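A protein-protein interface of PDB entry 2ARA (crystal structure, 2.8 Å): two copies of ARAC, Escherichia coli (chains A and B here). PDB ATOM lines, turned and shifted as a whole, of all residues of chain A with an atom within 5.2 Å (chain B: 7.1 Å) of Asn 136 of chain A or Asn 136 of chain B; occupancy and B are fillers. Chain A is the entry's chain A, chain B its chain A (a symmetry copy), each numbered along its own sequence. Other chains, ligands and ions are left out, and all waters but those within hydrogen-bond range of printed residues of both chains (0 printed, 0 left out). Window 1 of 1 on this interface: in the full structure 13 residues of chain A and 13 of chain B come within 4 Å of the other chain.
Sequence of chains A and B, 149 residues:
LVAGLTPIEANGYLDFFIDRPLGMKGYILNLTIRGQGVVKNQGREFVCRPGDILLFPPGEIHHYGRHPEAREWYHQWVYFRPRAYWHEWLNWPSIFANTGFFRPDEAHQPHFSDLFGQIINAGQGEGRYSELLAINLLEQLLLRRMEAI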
ATOM      1  N   LEU A 132      11.459   6.904  16.326  1.00  0.00           N
ATOM      2  CA  LEU A 132      11.486   7.850  17.436  1.00  0.00           C
ATOM      3  C   LEU A 132      10.725   9.144  17.102  1.00  0.00           C
ATOM      4  O   LEU A 132      10.082   9.726  17.970  1.00  0.00           O
ATOM      5  CB  LEU A 132      12.950   8.200  17.729  1.00  0.00           C
ATOM      6  CG  LEU A 132      13.856   7.112  18.329  1.00  0.00           C
ATOM      7  CD1 LEU A 132      15.271   7.522  18.143  1.00  0.00           C
ATOM      8  CD2 LEU A 132      13.534   6.838  19.836  1.00  0.00           C
ATOM      9  N   LEU A 133      10.877   9.654  15.890  1.00  0.00           N
ATOM     10  CA  LEU A 133      10.188  10.870  15.536  1.00  0.00           C
ATOM     11  C   LEU A 133       8.692  10.606  15.663  1.00  0.00           C
ATOM     12  O   LEU A 133       7.939  11.466  16.112  1.00  0.00           O
ATOM     13  CB  LEU A 133      10.546  11.321  14.114  1.00  0.00           C
ATOM     14  CG  LEU A 133      10.900  12.795  13.943  1.00  0.00           C
ATOM     15  CD1 LEU A 133      11.175  13.042  12.479  1.00  0.00           C
ATOM     16  CD2 LEU A 133       9.773  13.703  14.436  1.00  0.00           C
ATOM     17  N   ALA A 134       8.270   9.401  15.317  1.00  0.00           N
ATOM     18  CA  ALA A 134       6.865   9.067  15.401  1.00  0.00           C
ATOM     19  C   ALA A 134       6.480   9.157  16.848  1.00  0.00           C
ATOM     20  O   ALA A 134       5.434   9.723  17.203  1.00  0.00           O
ATOM     21  CB  ALA A 134       6.611   7.664  14.870  1.00  0.00           C
ATOM     22  N   ILE A 135       7.332   8.568  17.680  1.00  0.00           N
ATOM     23  CA  ILE A 135       7.125   8.581  19.119  1.00  0.00           C
ATOM     24  C   ILE A 135       7.122  10.026  19.627  1.00  0.00           C
ATOM     25  O   ILE A 135       6.225  10.391  20.388  1.00  0.00           O
ATOM     26  CB  ILE A 135       8.234   7.780  19.855  1.00  0.00           C
ATOM     27  CG1 ILE A 135       7.808   6.311  20.036  1.00  0.00           C
ATOM     28  CG2 ILE A 135       8.446   8.342  21.252  1.00  0.00           C
ATOM     29  CD1 ILE A 135       6.817   6.125  21.241  1.00  0.00           C
ATOM     30  N   ASN A 136       8.063  10.830  19.108  1.00  0.00           N
ATOM     31  CA  ASN A 136       8.277  12.245  19.449  1.00  0.00           C
ATOM     32  C   ASN A 136       7.138  13.103  19.030  1.00  0.00           C
ATOM     33  O   ASN A 136       6.791  14.044  19.748  1.00  0.00           O
ATOM     34  CB  ASN A 136       9.538  12.802  18.790  1.00  0.00           C
ATOM     35  CG  ASN A 136       9.618  14.329  18.866  1.00  0.00           C
ATOM     36  OD1 ASN A 136       9.291  15.009  17.901  1.00  0.00           O
ATOM     37  ND2 ASN A 136      10.124  14.864  19.979  1.00  0.00           N
ATOM     38  N   LEU A 137       6.568  12.787  17.863  1.00  0.00           N
ATOM     39  CA  LEU A 137       5.437  13.524  17.328  1.00  0.00           C
ATOM     40  C   LEU A 137       4.194  13.079  18.080  1.00  0.00           C
ATOM     41  O   LEU A 137       3.374  13.921  18.474  1.00  0.00           O
ATOM     42  CB  LEU A 137       5.308  13.316  15.826  1.00  0.00           C
ATOM     43  CG  LEU A 137       6.388  14.048  14.988  1.00  0.00           C
ATOM     44  CD1 LEU A 137       6.190  13.722  13.545  1.00  0.00           C
ATOM     45  CD2 LEU A 137       6.350  15.542  15.156  1.00  0.00           C
ATOM     46  N   LEU A 138       4.113  11.779  18.375  1.00  0.00           N
ATOM     47  CA  LEU A 138       2.986  11.247  19.158  1.00  0.00           C
ATOM     48  C   LEU A 138       2.978  12.046  20.495  1.00  0.00           C
ATOM     49  O   LEU A 138       1.929  12.456  21.014  1.00  0.00           O
ATOM     50  CB  LEU A 138       3.121   9.705  19.333  1.00  0.00           C
ATOM     51  CG  LEU A 138       2.252   9.103  20.424  1.00  0.00           C
ATOM     52  CD1 LEU A 138       0.842   9.601  20.470  1.00  0.00           C
ATOM     53  CD2 LEU A 138       2.324   7.667  20.267  1.00  0.00           C
ATOM     54  N   GLU A 139       4.180  12.361  20.973  1.00  0.00           N
ATOM     55  CA  GLU A 139       4.352  13.135  22.190  1.00  0.00           C
ATOM     56  C   GLU A 139       3.806  14.516  21.976  1.00  0.00           C
ATOM     57  O   GLU A 139       2.908  14.935  22.688  1.00  0.00           O
ATOM     58  CB  GLU A 139       5.835  13.218  22.545  1.00  0.00           C
ATOM     59  CG  GLU A 139       6.188  14.161  23.687  1.00  0.00           C
ATOM     60  CD  GLU A 139       7.362  13.662  24.513  1.00  0.00           C
ATOM     61  OE1 GLU A 139       8.472  13.537  23.974  1.00  0.00           O
ATOM     62  OE2 GLU A 139       7.191  13.368  25.707  1.00  0.00           O
ATOM     63  N   GLN A 140       4.380  15.238  21.008  1.00  0.00           N
ATOM     64  CA  GLN A 140       3.943  16.598  20.680  1.00  0.00           C
ATOM     65  C   GLN A 140       2.419  16.703  20.538  1.00  0.00           C
ATOM     66  O   GLN A 140       1.798  17.627  21.065  1.00  0.00           O
ATOM     67  CB  GLN A 140       4.608  17.061  19.388  1.00  0.00           C
ATOM     68  CG  GLN A 140       4.056  18.378  18.867  1.00  0.00           C
ATOM     69  CD  GLN A 140       4.881  18.971  17.731  1.00  0.00           C
ATOM     70  OE1 GLN A 140       4.443  19.906  17.042  1.00  0.00           O
ATOM     71  NE2 GLN A 140       6.105  18.472  17.572  1.00  0.00           N
ATOM     72  N   LEU A 143       0.671  16.671  23.949  1.00  0.00           N
ATOM     73  CA  LEU A 143       0.951  17.965  24.587  1.00  0.00           C
ATOM     74  C   LEU A 143      -0.024  19.005  24.007  1.00  0.00           C
ATOM     75  O   LEU A 143      -0.720  19.731  24.744  1.00  0.00           O
ATOM     76  CB  LEU A 143       2.414  18.419  24.389  1.00  0.00           C
ATOM     77  CG  LEU A 143       3.485  17.721  25.238  1.00  0.00           C
ATOM     78  CD1 LEU A 143       4.840  18.275  24.823  1.00  0.00           C
ATOM     79  CD2 LEU A 143       3.251  17.871  26.779  1.00  0.00           C
ATOM     80  N   LEU B   1      14.459  23.682  30.720  1.00  0.00           N
ATOM     81  CA  LEU B   1      14.416  24.579  29.532  1.00  0.00           C
ATOM     82  C   LEU B   1      13.977  25.965  29.910  1.00  0.00           C
ATOM     83  O   LEU B   1      12.956  26.166  30.600  1.00  0.00           O
ATOM     84  CB  LEU B   1      13.576  23.962  28.394  1.00  0.00           C
ATOM     85  CG  LEU B   1      14.241  22.856  27.633  1.00  0.00           C
ATOM     86  CD1 LEU B   1      15.145  23.462  26.614  1.00  0.00           C
ATOM     87  CD2 LEU B   1      15.058  22.043  28.594  1.00  0.00           C
ATOM     88  N   ARG B  83      17.523  14.729  28.556  1.00  0.00           N
ATOM     89  CA  ARG B  83      16.730  13.567  28.937  1.00  0.00           C
ATOM     90  C   ARG B  83      17.621  12.368  28.789  1.00  0.00           C
ATOM     91  O   ARG B  83      18.561  12.383  27.965  1.00  0.00           O
ATOM     92  CB  ARG B  83      15.497  13.345  28.051  1.00  0.00           C
ATOM     93  CG  ARG B  83      14.188  13.840  28.644  1.00  0.00           C
ATOM     94  CD  ARG B  83      12.994  13.534  27.751  1.00  0.00           C
ATOM     95  NE  ARG B  83      11.976  14.602  27.725  1.00  0.00           N
ATOM     96  CZ  ARG B  83      10.982  14.735  28.607  1.00  0.00           C
ATOM     97  NH1 ARG B  83      10.862  13.885  29.608  1.00  0.00           N
ATOM     98  NH2 ARG B  83      10.067  15.685  28.450  1.00  0.00           N
ATOM     99  N   TRP B  86      18.421  10.980  25.267  1.00  0.00           N
ATOM    100  CA  TRP B  86      19.035  12.088  24.542  1.00  0.00           C
ATOM    101  C   TRP B  86      20.533  11.954  24.410  1.00  0.00           C
ATOM    102  O   TRP B  86      21.068  12.269  23.369  1.00  0.00           O
ATOM    103  CB  TRP B  86      18.734  13.406  25.245  1.00  0.00           C
ATOM    104  CG  TRP B  86      17.301  13.825  25.183  1.00  0.00           C
ATOM    105  CD1 TRP B  86      16.220  13.019  25.016  1.00  0.00           C
ATOM    106  CD2 TRP B  86      16.812  15.175  25.253  1.00  0.00           C
ATOM    107  NE1 TRP B  86      15.068  13.780  24.967  1.00  0.00           N
ATOM    108  CE2 TRP B  86      15.392  15.103  25.103  1.00  0.00           C
ATOM    109  CE3 TRP B  86      17.403  16.446  25.427  1.00  0.00           C
ATOM    110  CZ2 TRP B  86      14.581  16.241  25.118  1.00  0.00           C
ATOM    111  CZ3 TRP B  86      16.593  17.586  25.444  1.00  0.00           C
ATOM    112  CH2 TRP B  86      15.189  17.469  25.287  1.00  0.00           C
ATOM    113  N   LEU B 115      12.996  25.250  13.460  1.00  0.00           N
ATOM    114  CA  LEU B 115      12.624  24.308  14.509  1.00  0.00           C
ATOM    115  C   LEU B 115      13.311  24.780  15.811  1.00  0.00           C
ATOM    116  O   LEU B 115      12.730  24.736  16.904  1.00  0.00           O
ATOM    117  CB  LEU B 115      13.024  22.880  14.129  1.00  0.00           C
ATOM    118  CG  LEU B 115      12.340  21.817  14.977  1.00  0.00           C
ATOM    119  CD1 LEU B 115      13.253  21.243  15.940  1.00  0.00           C
ATOM    120  CD2 LEU B 115      11.207  22.392  15.721  1.00  0.00           C
ATOM    121  N   ILE B 119      11.642  26.324  19.616  1.00  0.00           N
ATOM    122  CA  ILE B 119      12.007  25.942  20.968  1.00  0.00           C
ATOM    123  C   ILE B 119      12.005  27.178  21.817  1.00  0.00           C
ATOM    124  O   ILE B 119      11.263  27.201  22.793  1.00  0.00           O
ATOM    125  CB  ILE B 119      13.396  25.321  21.055  1.00  0.00           C
ATOM    126  CG1 ILE B 119      13.447  23.995  20.287  1.00  0.00           C
ATOM    127  CG2 ILE B 119      13.710  25.025  22.492  1.00  0.00           C
ATOM    128  CD1 ILE B 119      14.887  23.625  19.793  1.00  0.00           C
ATOM    129  N   SER B 130       3.764  24.612  28.135  1.00  0.00           N
ATOM    130  CA  SER B 130       4.761  25.125  27.202  1.00  0.00           C
ATOM    131  C   SER B 130       6.224  24.777  27.511  1.00  0.00           C
ATOM    132  O   SER B 130       7.023  24.672  26.586  1.00  0.00           O
ATOM    133  CB  SER B 130       4.585  26.637  26.942  1.00  0.00           C
ATOM    134  OG  SER B 130       4.605  27.373  28.137  1.00  0.00           O
ATOM    135  N   GLU B 131       6.566  24.521  28.782  1.00  0.00           N
ATOM    136  CA  GLU B 131       7.959  24.165  29.139  1.00  0.00           C
ATOM    137  C   GLU B 131       8.332  22.818  28.512  1.00  0.00           C
ATOM    138  O   GLU B 131       9.464  22.592  28.110  1.00  0.00           O
ATOM    139  CB  GLU B 131       8.158  24.118  30.677  1.00  0.00           C
ATOM    140  N   LEU B 132       7.358  21.923  28.478  1.00  0.00           N
ATOM    141  CA  LEU B 132       7.519  20.590  27.911  1.00  0.00           C
ATOM    142  C   LEU B 132       7.638  20.631  26.378  1.00  0.00           C
ATOM    143  O   LEU B 132       8.377  19.846  25.793  1.00  0.00           O
ATOM    144  CB  LEU B 132       6.286  19.760  28.289  1.00  0.00           C
ATOM    145  CG  LEU B 132       6.094  19.365  29.764  1.00  0.00           C
ATOM    146  CD1 LEU B 132       4.683  18.948  29.959  1.00  0.00           C
ATOM    147  CD2 LEU B 132       7.089  18.242  30.209  1.00  0.00           C
ATOM    148  N   LEU B 133       6.841  21.458  25.720  1.00  0.00           N
ATOM    149  CA  LEU B 133       6.913  21.523  24.282  1.00  0.00           C
ATOM    150  C   LEU B 133       8.324  21.962  23.910  1.00  0.00           C
ATOM    151  O   LEU B 133       8.898  21.476  22.939  1.00  0.00           O
ATOM    152  CB  LEU B 133       5.870  22.495  23.714  1.00  0.00           C
ATOM    153  CG  LEU B 133       5.050  21.989  22.532  1.00  0.00           C
ATOM    154  CD1 LEU B 133       4.121  23.098  22.098  1.00  0.00           C
ATOM    155  CD2 LEU B 133       5.947  21.559  21.370  1.00  0.00           C
ATOM    156  N   ALA B 134       8.904  22.842  24.710  1.00  0.00           N
ATOM    157  CA  ALA B 134      10.240  23.318  24.428  1.00  0.00           C
ATOM    158  C   ALA B 134      11.152  22.131  24.516  1.00  0.00           C
ATOM    159  O   ALA B 134      12.026  21.924  23.658  1.00  0.00           O
ATOM    160  CB  ALA B 134      10.656  24.383  25.432  1.00  0.00           C
ATOM    161  N   ILE B 135      10.954  21.362  25.581  1.00  0.00           N
ATOM    162  CA  ILE B 135      11.736  20.158  25.809  1.00  0.00           C
ATOM    163  C   ILE B 135      11.516  19.174  24.656  1.00  0.00           C
ATOM    164  O   ILE B 135      12.494  18.641  24.129  1.00  0.00           O
ATOM    165  CB  ILE B 135      11.341  19.476  27.148  1.00  0.00           C
ATOM    166  CG1 ILE B 135      12.225  19.992  28.298  1.00  0.00           C
ATOM    167  CG2 ILE B 135      11.580  17.977  27.062  1.00  0.00           C
ATOM    168  CD1 ILE B 135      13.637  19.304  28.316  1.00  0.00           C
ATOM    169  N   ASN B 136      10.250  19.046  24.230  1.00  0.00           N
ATOM    170  CA  ASN B 136       9.783  18.155  23.156  1.00  0.00           C
ATOM    171  C   ASN B 136      10.321  18.547  21.827  1.00  0.00           C
ATOM    172  O   ASN B 136      10.637  17.671  21.018  1.00  0.00           O
ATOM    173  CB  ASN B 136       8.260  18.145  23.050  1.00  0.00           C
ATOM    174  CG  ASN B 136       7.762  17.485  21.762  1.00  0.00           C
ATOM    175  OD1 ASN B 136       7.428  18.177  20.808  1.00  0.00           O
ATOM    176  ND2 ASN B 136       7.638  16.156  21.759  1.00  0.00           N
ATOM    177  N   LEU B 137      10.410  19.861  21.598  1.00  0.00           N
ATOM    178  CA  LEU B 137      10.929  20.398  20.353  1.00  0.00           C
ATOM    179  C   LEU B 137      12.441  20.279  20.388  1.00  0.00           C
ATOM    180  O   LEU B 137      13.055  19.867  19.392  1.00  0.00           O
ATOM    181  CB  LEU B 137      10.466  21.832  20.140  1.00  0.00           C
ATOM    182  CG  LEU B 137       8.968  21.968  19.764  1.00  0.00           C
ATOM    183  CD1 LEU B 137       8.626  23.416  19.637  1.00  0.00           C
ATOM    184  CD2 LEU B 137       8.620  21.276  18.474  1.00  0.00           C
ATOM    185  N   LEU B 138      13.029  20.529  21.562  1.00  0.00           N
ATOM    186  CA  LEU B 138      14.484  20.381  21.731  1.00  0.00           C
ATOM    187  C   LEU B 138      14.814  18.912  21.330  1.00  0.00           C
ATOM    188  O   LEU B 138      15.805  18.621  20.644  1.00  0.00           O
ATOM    189  CB  LEU B 138      14.908  20.761  23.181  1.00  0.00           C
ATOM    190  CG  LEU B 138      16.293  20.291  23.588  1.00  0.00           C
ATOM    191  CD1 LEU B 138      17.367  20.491  22.566  1.00  0.00           C
ATOM    192  CD2 LEU B 138      16.599  20.941  24.844  1.00  0.00           C
ATOM    193  N   GLU B 139      13.894  18.013  21.670  1.00  0.00           N
ATOM    194  CA  GLU B 139      14.027  16.604  21.339  1.00  0.00           C
ATOM    195  C   GLU B 139      13.986  16.443  19.848  1.00  0.00           C
ATOM    196  O   GLU B 139      14.928  15.933  19.263  1.00  0.00           O
ATOM    197  CB  GLU B 139      12.885  15.814  21.973  1.00  0.00           C
ATOM    198  CG  GLU B 139      12.780  14.354  21.555  1.00  0.00           C
ATOM    199  CD  GLU B 139      12.277  13.460  22.676  1.00  0.00           C
ATOM    200  OE1 GLU B 139      11.139  13.644  23.133  1.00  0.00           O
ATOM    201  OE2 GLU B 139      13.016  12.573  23.133  1.00  0.00           O
ATOM    202  N   GLN B 140      12.868  16.849  19.238  1.00  0.00           N
ATOM    203  CA  GLN B 140      12.691  16.762  17.785  1.00  0.00           C
ATOM    204  C   GLN B 140      13.903  17.308  17.017  1.00  0.00           C
ATOM    205  O   GLN B 140      14.377  16.690  16.063  1.00  0.00           O
ATOM    206  CB  GLN B 140      11.438  17.522  17.367  1.00  0.00           C
ATOM    207  CG  GLN B 140      11.292  17.656  15.860  1.00  0.00           C
ATOM    208  CD  GLN B 140       9.927  18.182  15.429  1.00  0.00           C
ATOM    209  OE1 GLN B 140       9.728  18.571  14.267  1.00  0.00           O
ATOM    210  NE2 GLN B 140       8.965  18.138  16.348  1.00  0.00           N
ATOM    211  N   LEU B 141      14.436  18.435  17.474  1.00  0.00           N
ATOM    212  CA  LEU B 141      15.589  19.067  16.829  1.00  0.00           C
ATOM    213  C   LEU B 141      16.756  18.102  16.700  1.00  0.00           C
ATOM    214  O   LEU B 141      17.298  17.915  15.618  1.00  0.00           O
ATOM    215  CB  LEU B 141      16.065  20.314  17.603  1.00  0.00           C
ATOM    216  CG  LEU B 141      17.176  21.044  16.813  1.00  0.00           C
ATOM    217  CD1 LEU B 141      16.505  21.784  15.677  1.00  0.00           C
ATOM    218  CD2 LEU B 141      17.978  21.998  17.623  1.00  0.00           C
ATOM    219  N   LEU B 143      16.848  14.855  17.081  1.00  0.00           N
ATOM    220  CA  LEU B 143      16.486  13.729  16.209  1.00  0.00           C
ATOM    221  C   LEU B 143      16.761  14.145  14.752  1.00  0.00           C
ATOM    222  O   LEU B 143      17.447  13.438  13.988  1.00  0.00           O
ATOM    223  CB  LEU B 143      15.015  13.291  16.383  1.00  0.00           C
ATOM    224  CG  LEU B 143      14.670  12.483  17.642  1.00  0.00           C
ATOM    225  CD1 LEU B 143      13.170  12.232  17.634  1.00  0.00           C
ATOM    226  CD2 LEU B 143      15.476  11.146  17.761  1.00  0.00           C
ATOM    227  N   ARG B 144      16.304  15.348  14.416  1.00  0.00           N
ATOM    228  CA  ARG B 144      16.466  15.904  13.077  1.00  0.00           C
ATOM    229  C   ARG B 144      17.908  15.927  12.637  1.00  0.00           C
ATOM    230  O   ARG B 144      18.216  15.721  11.462  1.00  0.00           O
ATOM    231  CB  ARG B 144      15.930  17.324  13.029  1.00  0.00           C
ATOM    232  CG  ARG B 144      14.430  17.442  13.114  1.00  0.00           C
ATOM    233  CD  ARG B 144      13.765  16.839  11.908  1.00  0.00           C
ATOM    234  NE  ARG B 144      12.315  16.868  12.033  1.00  0.00           N
ATOM    235  CZ  ARG B 144      11.488  16.231  11.215  1.00  0.00           C
ATOM    236  NH1 ARG B 144      11.965  15.507  10.202  1.00  0.00           N
ATOM    237  NH2 ARG B 144      10.184  16.322  11.413  1.00  0.00           N
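O of Asn 136 of chain A lies within hydrogen-bond range of ND2 of Asn 136 of chain B.
ND2 of Asn 136 of chain A sits close to N of Gln 140 of chain B (3.5 Å).
The backbone NH (N) of Gln 140 of chain A sits close to the side-chain amide nitrogen (ND2) of Asn 136 of chain B (3.5 Å).
The side-chain amide nitrogen of Gln 140 of chain B sits close to the side-chain amide nitrogen of Gln 140 of chain A.
The side-chain carboxylate (OE1) of Glu 139 of chain A lies close to the side-chain carboxylate (OE1) of Glu 139 of chain B.
NE1 of Trp 86 of chain B lies within hydrogen-bond range of OE2 of Glu 139 of chain B (3.0 Å).
Leu 143 of chain B touches Leu 132 of chain A (CD2 to CD1, 3.6 Å).
Leu 143 of chain B touches Leu 133 of chain A (CD1 to N, 3.9 Å).
Arg 144 of chain B touches Leu 133 of chain A (CZ to CD1, 3.4 Å).
Asn 136 of chain A touches Glu 139 of chain B.
CD1 of Leu 143 of chain B touches CB of Asn 136 of chain A (3.9 Å).
Leu 137 of chain A touches Gln 140 of chain B.
Glu 139 of chain A touches Asn 136 of chain B (CG to ND2, 3.1 Å).
Leu 132 of chain B touches Leu 143 of chain A.
Leu 133 of chain B touches Leu 143 of chain A (N to CD1, 3.9 Å).
CB of Asn 136 of chain B touches CD1 of Leu 143 of chain A (3.9 Å).
Of the printed residues of chain B, Asn 136 of chain A touches Asn 136 (3.0 Å), Glu 139 (3.1 Å), Gln 140 (3.3 Å) and Leu 143 (3.9 Å).
Of chain A, only Asn 136, Glu 139, Gln 140 and Leu 143 come within 4 Å of Asn 136 of chain B.
Of the printed residues of chain A, Arg 144 of chain B touches Leu 133 (3.4 Å).
Of the printed residues of chain B, Leu 132 of chain A touches Leu 143 (3.6 Å).
Of the printed residues of chain A, Leu 132 of chain B touches Leu 143.
Of the printed residues of chain B, Glu 139 of chain A touches Asn 136 and Glu 139.
Of the printed residues of chain B, Leu 137 of chain A touches Gln 140 (3.9 Å).
The nearest residue of chain B that does not touch Asn 136 of chain A is Leu 137 of chain B (5.3 Å).
The nearest printed residue of chain B that does not touch Leu 132 of chain A is Glu 139 of chain B (6.4 Å).
Of the 19 printed residues of chain B, 8 touch a printed residue of chain A.
Printed residues of chain B that touch a printed residue of chain A: Leu 132, Leu 133, Asn 136, Leu 137, Glu 139, Gln 140, Leu 143 and Arg 144.
Of the 10 printed residues of chain A, 7 touch a printed residue of chain B.
Printed residues of chain A that touch a printed residue of chain B: Leu 132, Leu 133, Asn 136, Leu 137, Glu 139, Gln 140 and Leu 143.
Leu 132 of chain A touches Leu 143 of chain B, and with the chains exchanged Leu 143 of chain A touches Leu 132 of chain B.
Leu 133 of chain A touches Leu 143 of chain B, and with the chains exchanged Leu 143 of chain A touches Leu 133 of chain B.
Asn 136 of chain A touches its own counterpart, Asn 136 of chain B.
Leu 137 of chain A touches Gln 140 of chain B, and with the chains exchanged Gln 140 of chain A touches Leu 137 of chain B.
Of the 16 pairs that touch across the chains among the printed residues, 15 have their exchanged pair printed and touching as well.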
